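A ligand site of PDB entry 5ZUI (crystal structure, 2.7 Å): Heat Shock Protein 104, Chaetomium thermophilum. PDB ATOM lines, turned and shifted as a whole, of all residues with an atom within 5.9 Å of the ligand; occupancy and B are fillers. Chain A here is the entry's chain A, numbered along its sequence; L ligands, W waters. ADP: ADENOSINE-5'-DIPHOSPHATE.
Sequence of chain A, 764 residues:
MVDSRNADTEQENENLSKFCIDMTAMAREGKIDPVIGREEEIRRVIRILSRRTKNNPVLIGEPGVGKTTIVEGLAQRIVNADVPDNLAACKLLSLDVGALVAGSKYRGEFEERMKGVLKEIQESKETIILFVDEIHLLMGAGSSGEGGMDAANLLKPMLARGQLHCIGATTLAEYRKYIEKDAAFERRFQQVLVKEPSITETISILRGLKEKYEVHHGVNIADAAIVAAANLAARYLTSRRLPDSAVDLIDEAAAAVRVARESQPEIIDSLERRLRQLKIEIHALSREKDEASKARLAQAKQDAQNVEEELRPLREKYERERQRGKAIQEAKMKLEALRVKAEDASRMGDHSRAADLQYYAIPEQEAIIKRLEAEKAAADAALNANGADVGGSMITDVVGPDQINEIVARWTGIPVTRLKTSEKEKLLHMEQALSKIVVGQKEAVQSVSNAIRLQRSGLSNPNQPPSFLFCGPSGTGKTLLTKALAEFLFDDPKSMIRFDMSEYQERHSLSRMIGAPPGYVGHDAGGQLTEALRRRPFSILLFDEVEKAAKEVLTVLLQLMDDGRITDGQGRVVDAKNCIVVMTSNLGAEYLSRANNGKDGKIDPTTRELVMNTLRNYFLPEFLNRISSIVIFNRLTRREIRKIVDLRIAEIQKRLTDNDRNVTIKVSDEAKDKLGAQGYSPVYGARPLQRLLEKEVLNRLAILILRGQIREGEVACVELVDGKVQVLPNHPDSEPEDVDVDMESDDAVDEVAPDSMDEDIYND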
ATOM      1  N   ASP A  33      17.988  19.436  21.424  1.00  0.00           N
ATOM      2  CA  ASP A  33      17.812  18.294  22.302  1.00  0.00           C
ATOM      3  C   ASP A  33      17.219  18.752  23.640  1.00  0.00           C
ATOM      4  O   ASP A  33      17.339  19.926  24.003  1.00  0.00           O
ATOM      5  CB  ASP A  33      19.143  17.575  22.533  1.00  0.00           C
ATOM      6  CG  ASP A  33      19.814  17.153  21.237  1.00  0.00           C
ATOM      7  OD1 ASP A  33      19.091  16.798  20.281  1.00  0.00           O
ATOM      8  OD2 ASP A  33      21.059  17.157  21.187  1.00  0.00           O
ATOM      9  N   PRO A  34      16.563  17.845  24.370  1.00  0.00           N
ATOM     10  CA  PRO A  34      15.923  18.260  25.626  1.00  0.00           C
ATOM     11  C   PRO A  34      16.900  18.826  26.650  1.00  0.00           C
ATOM     12  O   PRO A  34      18.099  18.513  26.642  1.00  0.00           O
ATOM     13  CB  PRO A  34      15.284  16.949  26.135  1.00  0.00           C
ATOM     14  CG  PRO A  34      15.884  15.856  25.320  1.00  0.00           C
ATOM     15  CD  PRO A  34      16.198  16.479  23.999  1.00  0.00           C
ATOM     16  N   VAL A  35      16.370  19.662  27.529  1.00  0.00           N
ATOM     17  CA  VAL A  35      17.103  20.235  28.652  1.00  0.00           C
ATOM     18  C   VAL A  35      16.560  19.603  29.930  1.00  0.00           C
ATOM     19  O   VAL A  35      15.339  19.647  30.171  1.00  0.00           O
ATOM     20  CB  VAL A  35      16.967  21.768  28.692  1.00  0.00           C
ATOM     21  CG1 VAL A  35      17.739  22.353  29.865  1.00  0.00           C
ATOM     22  CG2 VAL A  35      17.431  22.394  27.373  1.00  0.00           C
ATOM     23  N   ILE A  36      17.442  19.023  30.732  1.00  0.00           N
ATOM     24  CA  ILE A  36      17.067  18.307  31.940  1.00  0.00           C
ATOM     25  C   ILE A  36      17.539  19.117  33.146  1.00  0.00           C
ATOM     26  O   ILE A  36      18.724  19.453  33.256  1.00  0.00           O
ATOM     27  CB  ILE A  36      17.665  16.890  31.976  1.00  0.00           C
ATOM     28  CG1 ILE A  36      17.272  16.098  30.721  1.00  0.00           C
ATOM     29  CG2 ILE A  36      17.241  16.149  33.243  1.00  0.00           C
ATOM     30  CD1 ILE A  36      15.789  16.104  30.428  1.00  0.00           C
ATOM     31  N   GLY A  37      16.612  19.407  34.057  1.00  0.00           N
ATOM     32  CA  GLY A  37      16.929  20.154  35.261  1.00  0.00           C
ATOM     33  C   GLY A  37      17.285  21.598  34.943  1.00  0.00           C
ATOM     34  O   GLY A  37      16.794  22.205  33.985  1.00  0.00           O
ATOM     35  N   ARG A  38      18.164  22.150  35.786  1.00  0.00           N
ATOM     36  CA  ARG A  38      18.697  23.504  35.597  1.00  0.00           C
ATOM     37  C   ARG A  38      17.596  24.557  35.607  1.00  0.00           C
ATOM     38  O   ARG A  38      17.689  25.586  34.925  1.00  0.00           O
ATOM     39  CB  ARG A  38      19.547  23.578  34.326  1.00  0.00           C
ATOM     40  CG  ARG A  38      20.812  22.707  34.392  1.00  0.00           C
ATOM     41  CD  ARG A  38      22.014  23.425  33.792  1.00  0.00           C
ATOM     42  NE  ARG A  38      23.302  22.956  34.280  1.00  0.00           N
ATOM     43  CZ  ARG A  38      23.791  23.195  35.501  1.00  0.00           C
ATOM     44  NH1 ARG A  38      23.092  23.886  36.385  1.00  0.00           N
ATOM     45  NH2 ARG A  38      24.989  22.733  35.829  1.00  0.00           N
ATOM     46  N   GLY A  61      31.069  29.064  34.082  1.00  0.00           N
ATOM     47  CA  GLY A  61      31.259  27.684  34.456  1.00  0.00           C
ATOM     48  C   GLY A  61      32.315  27.031  33.617  1.00  0.00           C
ATOM     49  O   GLY A  61      32.706  27.534  32.553  1.00  0.00           O
ATOM     50  N   GLU A  62      32.786  25.873  34.099  1.00  0.00           N
ATOM     51  CA  GLU A  62      33.837  25.145  33.408  1.00  0.00           C
ATOM     52  C   GLU A  62      33.330  24.658  32.050  1.00  0.00           C
ATOM     53  O   GLU A  62      32.126  24.564  31.837  1.00  0.00           O
ATOM     54  CB  GLU A  62      34.316  23.977  34.260  1.00  0.00           C
ATOM     55  CG  GLU A  62      35.142  24.386  35.449  1.00  0.00           C
ATOM     56  CD  GLU A  62      36.261  25.351  35.074  1.00  0.00           C
ATOM     57  OE1 GLU A  62      37.135  24.953  34.290  1.00  0.00           O
ATOM     58  OE2 GLU A  62      36.252  26.491  35.576  1.00  0.00           O
ATOM     59  N   PRO A  63      34.236  24.376  31.119  1.00  0.00           N
ATOM     60  CA  PRO A  63      33.787  23.902  29.802  1.00  0.00           C
ATOM     61  C   PRO A  63      33.053  22.573  29.919  1.00  0.00           C
ATOM     62  O   PRO A  63      33.557  21.616  30.508  1.00  0.00           O
ATOM     63  CB  PRO A  63      35.102  23.761  29.019  1.00  0.00           C
ATOM     64  CG  PRO A  63      36.044  24.664  29.692  1.00  0.00           C
ATOM     65  CD  PRO A  63      35.682  24.605  31.157  1.00  0.00           C
ATOM     66  N   GLY A  64      31.847  22.539  29.348  1.00  0.00           N
ATOM     67  CA  GLY A  64      31.065  21.322  29.278  1.00  0.00           C
ATOM     68  C   GLY A  64      30.047  21.118  30.385  1.00  0.00           C
ATOM     69  O   GLY A  64      29.348  20.097  30.371  1.00  0.00           O
ATOM     70  N   VAL A  65      29.950  22.048  31.340  1.00  0.00           N
ATOM     71  CA  VAL A  65      28.978  21.899  32.418  1.00  0.00           C
ATOM     72  C   VAL A  65      27.546  22.163  31.983  1.00  0.00           C
ATOM     73  O   VAL A  65      26.619  21.866  32.737  1.00  0.00           O
ATOM     74  CB  VAL A  65      29.299  22.838  33.597  1.00  0.00           C
ATOM     75  CG1 VAL A  65      30.673  22.524  34.180  1.00  0.00           C
ATOM     76  CG2 VAL A  65      29.194  24.286  33.155  1.00  0.00           C
ATOM     77  N   GLY A  66      27.343  22.711  30.786  1.00  0.00           N
ATOM     78  CA  GLY A  66      26.007  22.915  30.280  1.00  0.00           C
ATOM     79  C   GLY A  66      25.587  24.370  30.116  1.00  0.00           C
ATOM     80  O   GLY A  66      24.390  24.664  30.064  1.00  0.00           O
ATOM     81  N   LYS A  67      26.556  25.286  30.029  1.00  0.00           N
ATOM     82  CA  LYS A  67      26.232  26.688  29.865  1.00  0.00           C
ATOM     83  C   LYS A  67      25.374  26.911  28.633  1.00  0.00           C
ATOM     84  O   LYS A  67      24.334  27.587  28.693  1.00  0.00           O
ATOM     85  CB  LYS A  67      27.507  27.538  29.799  1.00  0.00           C
ATOM     86  CG  LYS A  67      28.451  27.374  31.003  1.00  0.00           C
ATOM     87  CD  LYS A  67      29.704  28.253  30.887  1.00  0.00           C
ATOM     88  CE  LYS A  67      30.474  27.970  29.605  1.00  0.00           C
ATOM     89  NZ  LYS A  67      31.202  26.673  29.666  1.00  0.00           N
ATOM     90  N   THR A  68      25.765  26.331  27.500  1.00  0.00           N
ATOM     91  CA  THR A  68      25.017  26.553  26.270  1.00  0.00           C
ATOM     92  C   THR A  68      23.597  25.992  26.362  1.00  0.00           C
ATOM     93  O   THR A  68      22.634  26.646  25.962  1.00  0.00           O
ATOM     94  CB  THR A  68      25.742  25.943  25.068  1.00  0.00           C
ATOM     95  OG1 THR A  68      26.841  26.786  24.690  1.00  0.00           O
ATOM     96  CG2 THR A  68      24.783  25.804  23.896  1.00  0.00           C
ATOM     97  N   THR A  69      23.450  24.781  26.898  1.00  0.00           N
ATOM     98  CA  THR A  69      22.125  24.179  26.931  1.00  0.00           C
ATOM     99  C   THR A  69      21.179  24.939  27.854  1.00  0.00           C
ATOM    100  O   THR A  69      19.960  24.772  27.719  1.00  0.00           O
ATOM    101  CB  THR A  69      22.202  22.709  27.331  1.00  0.00           C
ATOM    102  OG1 THR A  69      22.964  22.559  28.534  1.00  0.00           O
ATOM    103  CG2 THR A  69      22.841  21.908  26.224  1.00  0.00           C
ATOM    104  N   ILE A  70      21.705  25.751  28.771  1.00  0.00           N
ATOM    105  CA  ILE A  70      20.850  26.643  29.548  1.00  0.00           C
ATOM    106  C   ILE A  70      20.193  27.678  28.631  1.00  0.00           C
ATOM    107  O   ILE A  70      18.981  27.887  28.676  1.00  0.00           O
ATOM    108  CB  ILE A  70      21.656  27.312  30.674  1.00  0.00           C
ATOM    109  CG1 ILE A  70      21.730  26.383  31.890  1.00  0.00           C
ATOM    110  CG2 ILE A  70      21.059  28.669  31.036  1.00  0.00           C
ATOM    111  CD1 ILE A  70      22.598  26.906  33.022  1.00  0.00           C
ATOM    112  N   ASP A 133      28.670  32.789  23.209  1.00  0.00           N
ATOM    113  CA  ASP A 133      29.473  31.832  23.960  1.00  0.00           C
ATOM    114  C   ASP A 133      30.948  32.217  23.853  1.00  0.00           C
ATOM    115  O   ASP A 133      31.377  32.851  22.873  1.00  0.00           O
ATOM    116  CB  ASP A 133      29.255  30.412  23.429  1.00  0.00           C
ATOM    117  CG  ASP A 133      30.065  29.365  24.188  1.00  0.00           C
ATOM    118  OD1 ASP A 133      29.930  29.271  25.425  1.00  0.00           O
ATOM    119  OD2 ASP A 133      30.845  28.634  23.534  1.00  0.00           O
ATOM    120  N   ILE A 205      20.464  13.553  33.299  1.00  0.00           N
ATOM    121  CA  ILE A 205      20.667  14.186  32.007  1.00  0.00           C
ATOM    122  C   ILE A 205      20.766  13.120  30.909  1.00  0.00           C
ATOM    123  O   ILE A 205      20.089  13.191  29.884  1.00  0.00           O
ATOM    124  CB  ILE A 205      21.906  15.091  32.033  1.00  0.00           C
ATOM    125  CG1 ILE A 205      21.691  16.231  33.052  1.00  0.00           C
ATOM    126  CG2 ILE A 205      22.187  15.643  30.649  1.00  0.00           C
ATOM    127  CD1 ILE A 205      22.878  17.158  33.198  1.00  0.00           C
ATOM    128  N   LEU A 209      18.325  12.339  27.786  1.00  0.00           N
ATOM    129  CA  LEU A 209      18.826  12.406  26.421  1.00  0.00           C
ATOM    130  C   LEU A 209      18.783  11.067  25.714  1.00  0.00           C
ATOM    131  O   LEU A 209      19.021  11.018  24.494  1.00  0.00           O
ATOM    132  CB  LEU A 209      20.267  12.937  26.418  1.00  0.00           C
ATOM    133  CG  LEU A 209      20.432  14.441  26.620  1.00  0.00           C
ATOM    134  CD1 LEU A 209      21.866  14.782  26.942  1.00  0.00           C
ATOM    135  CD2 LEU A 209      19.961  15.198  25.386  1.00  0.00           C
ATOM    136  N   TYR A 213      19.501  10.206  21.445  1.00  0.00           N
ATOM    137  CA  TYR A 213      20.694   9.555  20.927  1.00  0.00           C
ATOM    138  C   TYR A 213      20.425   8.141  20.415  1.00  0.00           C
ATOM    139  O   TYR A 213      21.218   7.626  19.628  1.00  0.00           O
ATOM    140  CB  TYR A 213      21.798   9.538  21.986  1.00  0.00           C
ATOM    141  CG  TYR A 213      22.553  10.843  22.078  1.00  0.00           C
ATOM    142  CD1 TYR A 213      23.729  11.030  21.352  1.00  0.00           C
ATOM    143  CD2 TYR A 213      22.097  11.888  22.863  1.00  0.00           C
ATOM    144  CE1 TYR A 213      24.422  12.230  21.411  1.00  0.00           C
ATOM    145  CE2 TYR A 213      22.780  13.087  22.941  1.00  0.00           C
ATOM    146  CZ  TYR A 213      23.948  13.253  22.215  1.00  0.00           C
ATOM    147  OH  TYR A 213      24.632  14.442  22.284  1.00  0.00           O
ATOM    148  N   PRO A 243      28.374  17.184  32.324  1.00  0.00           N
ATOM    149  CA  PRO A 243      28.067  15.858  31.795  1.00  0.00           C
ATOM    150  C   PRO A 243      28.662  15.633  30.413  1.00  0.00           C
ATOM    151  O   PRO A 243      28.497  14.539  29.872  1.00  0.00           O
ATOM    152  CB  PRO A 243      26.542  15.864  31.742  1.00  0.00           C
ATOM    153  CG  PRO A 243      26.217  17.291  31.398  1.00  0.00           C
ATOM    154  CD  PRO A 243      27.313  18.159  32.012  1.00  0.00           C
ATOM    155  N   ASP A 244      29.327  16.646  29.856  1.00  0.00           N
ATOM    156  CA  ASP A 244      29.924  16.520  28.527  1.00  0.00           C
ATOM    157  C   ASP A 244      30.800  15.280  28.431  1.00  0.00           C
ATOM    158  O   ASP A 244      30.750  14.550  27.430  1.00  0.00           O
ATOM    159  CB  ASP A 244      30.726  17.780  28.198  1.00  0.00           C
ATOM    160  CG  ASP A 244      31.076  17.868  26.723  1.00  0.00           C
ATOM    161  OD1 ASP A 244      30.232  17.499  25.875  1.00  0.00           O
ATOM    162  OD2 ASP A 244      32.206  18.321  26.415  1.00  0.00           O
ATOM    163  N   VAL A 247      28.472  12.518  28.055  1.00  0.00           N
ATOM    164  CA  VAL A 247      27.778  12.585  26.781  1.00  0.00           C
ATOM    165  C   VAL A 247      28.689  12.149  25.636  1.00  0.00           C
ATOM    166  O   VAL A 247      28.325  11.317  24.810  1.00  0.00           O
ATOM    167  CB  VAL A 247      27.202  13.999  26.545  1.00  0.00           C
ATOM    168  CG1 VAL A 247      26.839  14.209  25.077  1.00  0.00           C
ATOM    169  CG2 VAL A 247      25.980  14.226  27.431  1.00  0.00           C
ATOM    170  N   ASP A 248      29.907  12.713  25.582  1.00  0.00           N
ATOM    171  CA  ASP A 248      30.865  12.307  24.558  1.00  0.00           C
ATOM    172  C   ASP A 248      31.148  10.813  24.620  1.00  0.00           C
ATOM    173  O   ASP A 248      31.391  10.189  23.574  1.00  0.00           O
ATOM    174  CB  ASP A 248      32.184  13.085  24.711  1.00  0.00           C
ATOM    175  CG  ASP A 248      32.150  14.435  24.027  1.00  0.00           C
ATOM    176  OD1 ASP A 248      31.038  14.943  23.731  1.00  0.00           O
ATOM    177  OD2 ASP A 248      33.240  15.003  23.792  1.00  0.00           O
HETATM  178  PB  ADP L   1      29.111  24.281  27.812  1.00  0.00           P
HETATM  179  O1B ADP L   1      28.283  25.082  26.837  1.00  0.00           O
HETATM  180  O2B ADP L   1      29.008  24.736  29.244  1.00  0.00           O
HETATM  181  O3B ADP L   1      30.523  24.009  27.336  1.00  0.00           O
HETATM  182  PA  ADP L   1      27.185  22.451  26.866  1.00  0.00           P
HETATM  183  O1A ADP L   1      27.673  22.559  25.442  1.00  0.00           O
HETATM  184  O2A ADP L   1      25.917  23.168  27.265  1.00  0.00           O
HETATM  185  O3A ADP L   1      28.397  22.836  27.847  1.00  0.00           O
HETATM  186  O5' ADP L   1      27.029  20.883  27.222  1.00  0.00           O
HETATM  187  C5' ADP L   1      27.789  19.910  26.511  1.00  0.00           C
HETATM  188  C4' ADP L   1      26.962  18.652  26.350  1.00  0.00           C
HETATM  189  O4' ADP L   1      26.291  18.353  27.577  1.00  0.00           O
HETATM  190  C3' ADP L   1      25.903  18.854  25.276  1.00  0.00           C
HETATM  191  O3' ADP L   1      25.971  17.780  24.337  1.00  0.00           O
HETATM  192  C2' ADP L   1      24.583  18.815  26.014  1.00  0.00           C
HETATM  193  O2' ADP L   1      23.631  18.043  25.285  1.00  0.00           O
HETATM  194  C1' ADP L   1      24.893  18.173  27.360  1.00  0.00           C
HETATM  195  N9  ADP L   1      24.127  18.803  28.461  1.00  0.00           N
HETATM  196  C8  ADP L   1      24.608  19.661  29.379  1.00  0.00           C
HETATM  197  N7  ADP L   1      23.645  20.040  30.262  1.00  0.00           N
HETATM  198  C5  ADP L   1      22.507  19.404  29.895  1.00  0.00           C
HETATM  199  C6  ADP L   1      21.112  19.345  30.391  1.00  0.00           C
HETATM  200  N6  ADP L   1      20.710  20.066  31.468  1.00  0.00           N
HETATM  201  N1  ADP L   1      20.240  18.558  29.722  1.00  0.00           N
HETATM  202  C2  ADP L   1      20.612  17.845  28.646  1.00  0.00           C
HETATM  203  N3  ADP L   1      21.861  17.851  28.146  1.00  0.00           N
HETATM  204  C4  ADP L   1      22.837  18.589  28.715  1.00  0.00           C
HETATM  205  O   HOH W   1      31.623  26.393  25.300  1.00  0.00           O
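The backbone NH (N) of Lys 67 sits at hydrogen-bond distance from an oxygen (O2B) of the ligand.
The side-chain amino group (NZ) of Lys 67 is in salt-bridge range of an oxygen (O2B) of the ligand.
N of Ile 36 sits at hydrogen-bond distance from N1 of the ligand (3.0 Å).
A nitrogen (N6) of the ligand sits at hydrogen-bond distance from the backbone carbonyl oxygen (O) of Ile 36 (2.7 Å).
The backbone NH (N) of Gly 64 is in hydrogen-bond range of an oxygen (O3B) of the ligand, 2.8 Å away.
N of Thr 68 is in hydrogen-bond range of O1B of the ligand (2.9 Å).
The side-chain hydroxyl of Thr 68 sits at hydrogen-bond distance from an oxygen (O1B) of the ligand.
An oxygen (O2A) of the ligand sits at hydrogen-bond distance from the backbone NH of Thr 69 (3.0 Å).
N7 of the ligand sits at hydrogen-bond distance from OG1 of Thr 69 (3.1 Å).
The backbone NH of Gly 66 is in hydrogen-bond range of an oxygen (O2B) of the ligand, 3.0 Å away.
NZ of Lys 67 lies within hydrogen-bond range of O of Glu 62.
The side-chain amino group (NZ) of Lys 67 is in hydrogen-bond range of the backbone carbonyl oxygen (O) of Gly 61 (3.4 Å).
The backbone carbonyl oxygen (O) of Gly 64 lies close to the backbone NH (N) of Asp 244 (3.5 Å).
OG1 of Thr 69 lies within hydrogen-bond range of O of Gly 66 (3.0 Å).
Pro 34 touches the ligand (O to C2, 3.3 Å).
Val 35 touches the ligand (CA to N1, 3.7 Å).
Arg 38 touches the ligand.
C of Pro 63 touches O3B of the ligand, at 3.9 Å.
Val 65 touches the ligand (N to O2B, 3.5 Å).
Ile 205 touches the ligand.
Leu 209 touches the ligand (CD1 to N3, 3.3 Å).
Pro 243 touches the ligand (CG to C8, 3.5 Å).
OD1 of Asp 244 touches C5' of the ligand, at 3.5 Å.
Val 247 touches the ligand (CG1 to O3', 3.7 Å).
Hydrophobic or aromatic side chains that line the ligand: Ile 36, Val 65, Ile 205, Leu 209, Pro 243 and Val 247.
16 residues have an atom within 4 Å of the ligand: Pro 34, Val 35, Ile 36, Arg 38, Pro 63, Gly 64, Val 65, Gly 66, Lys 67, Thr 68, Thr 69, Ile 205, Leu 209, Pro 243, Asp 244 and Val 247.
The nearest printed residue that does not touch the ligand is Glu 62 (4.1 Å).
Water W1 bridges OD2 of Asp 133 (3.0 Å) and O3B of the ligand (3.3 Å).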
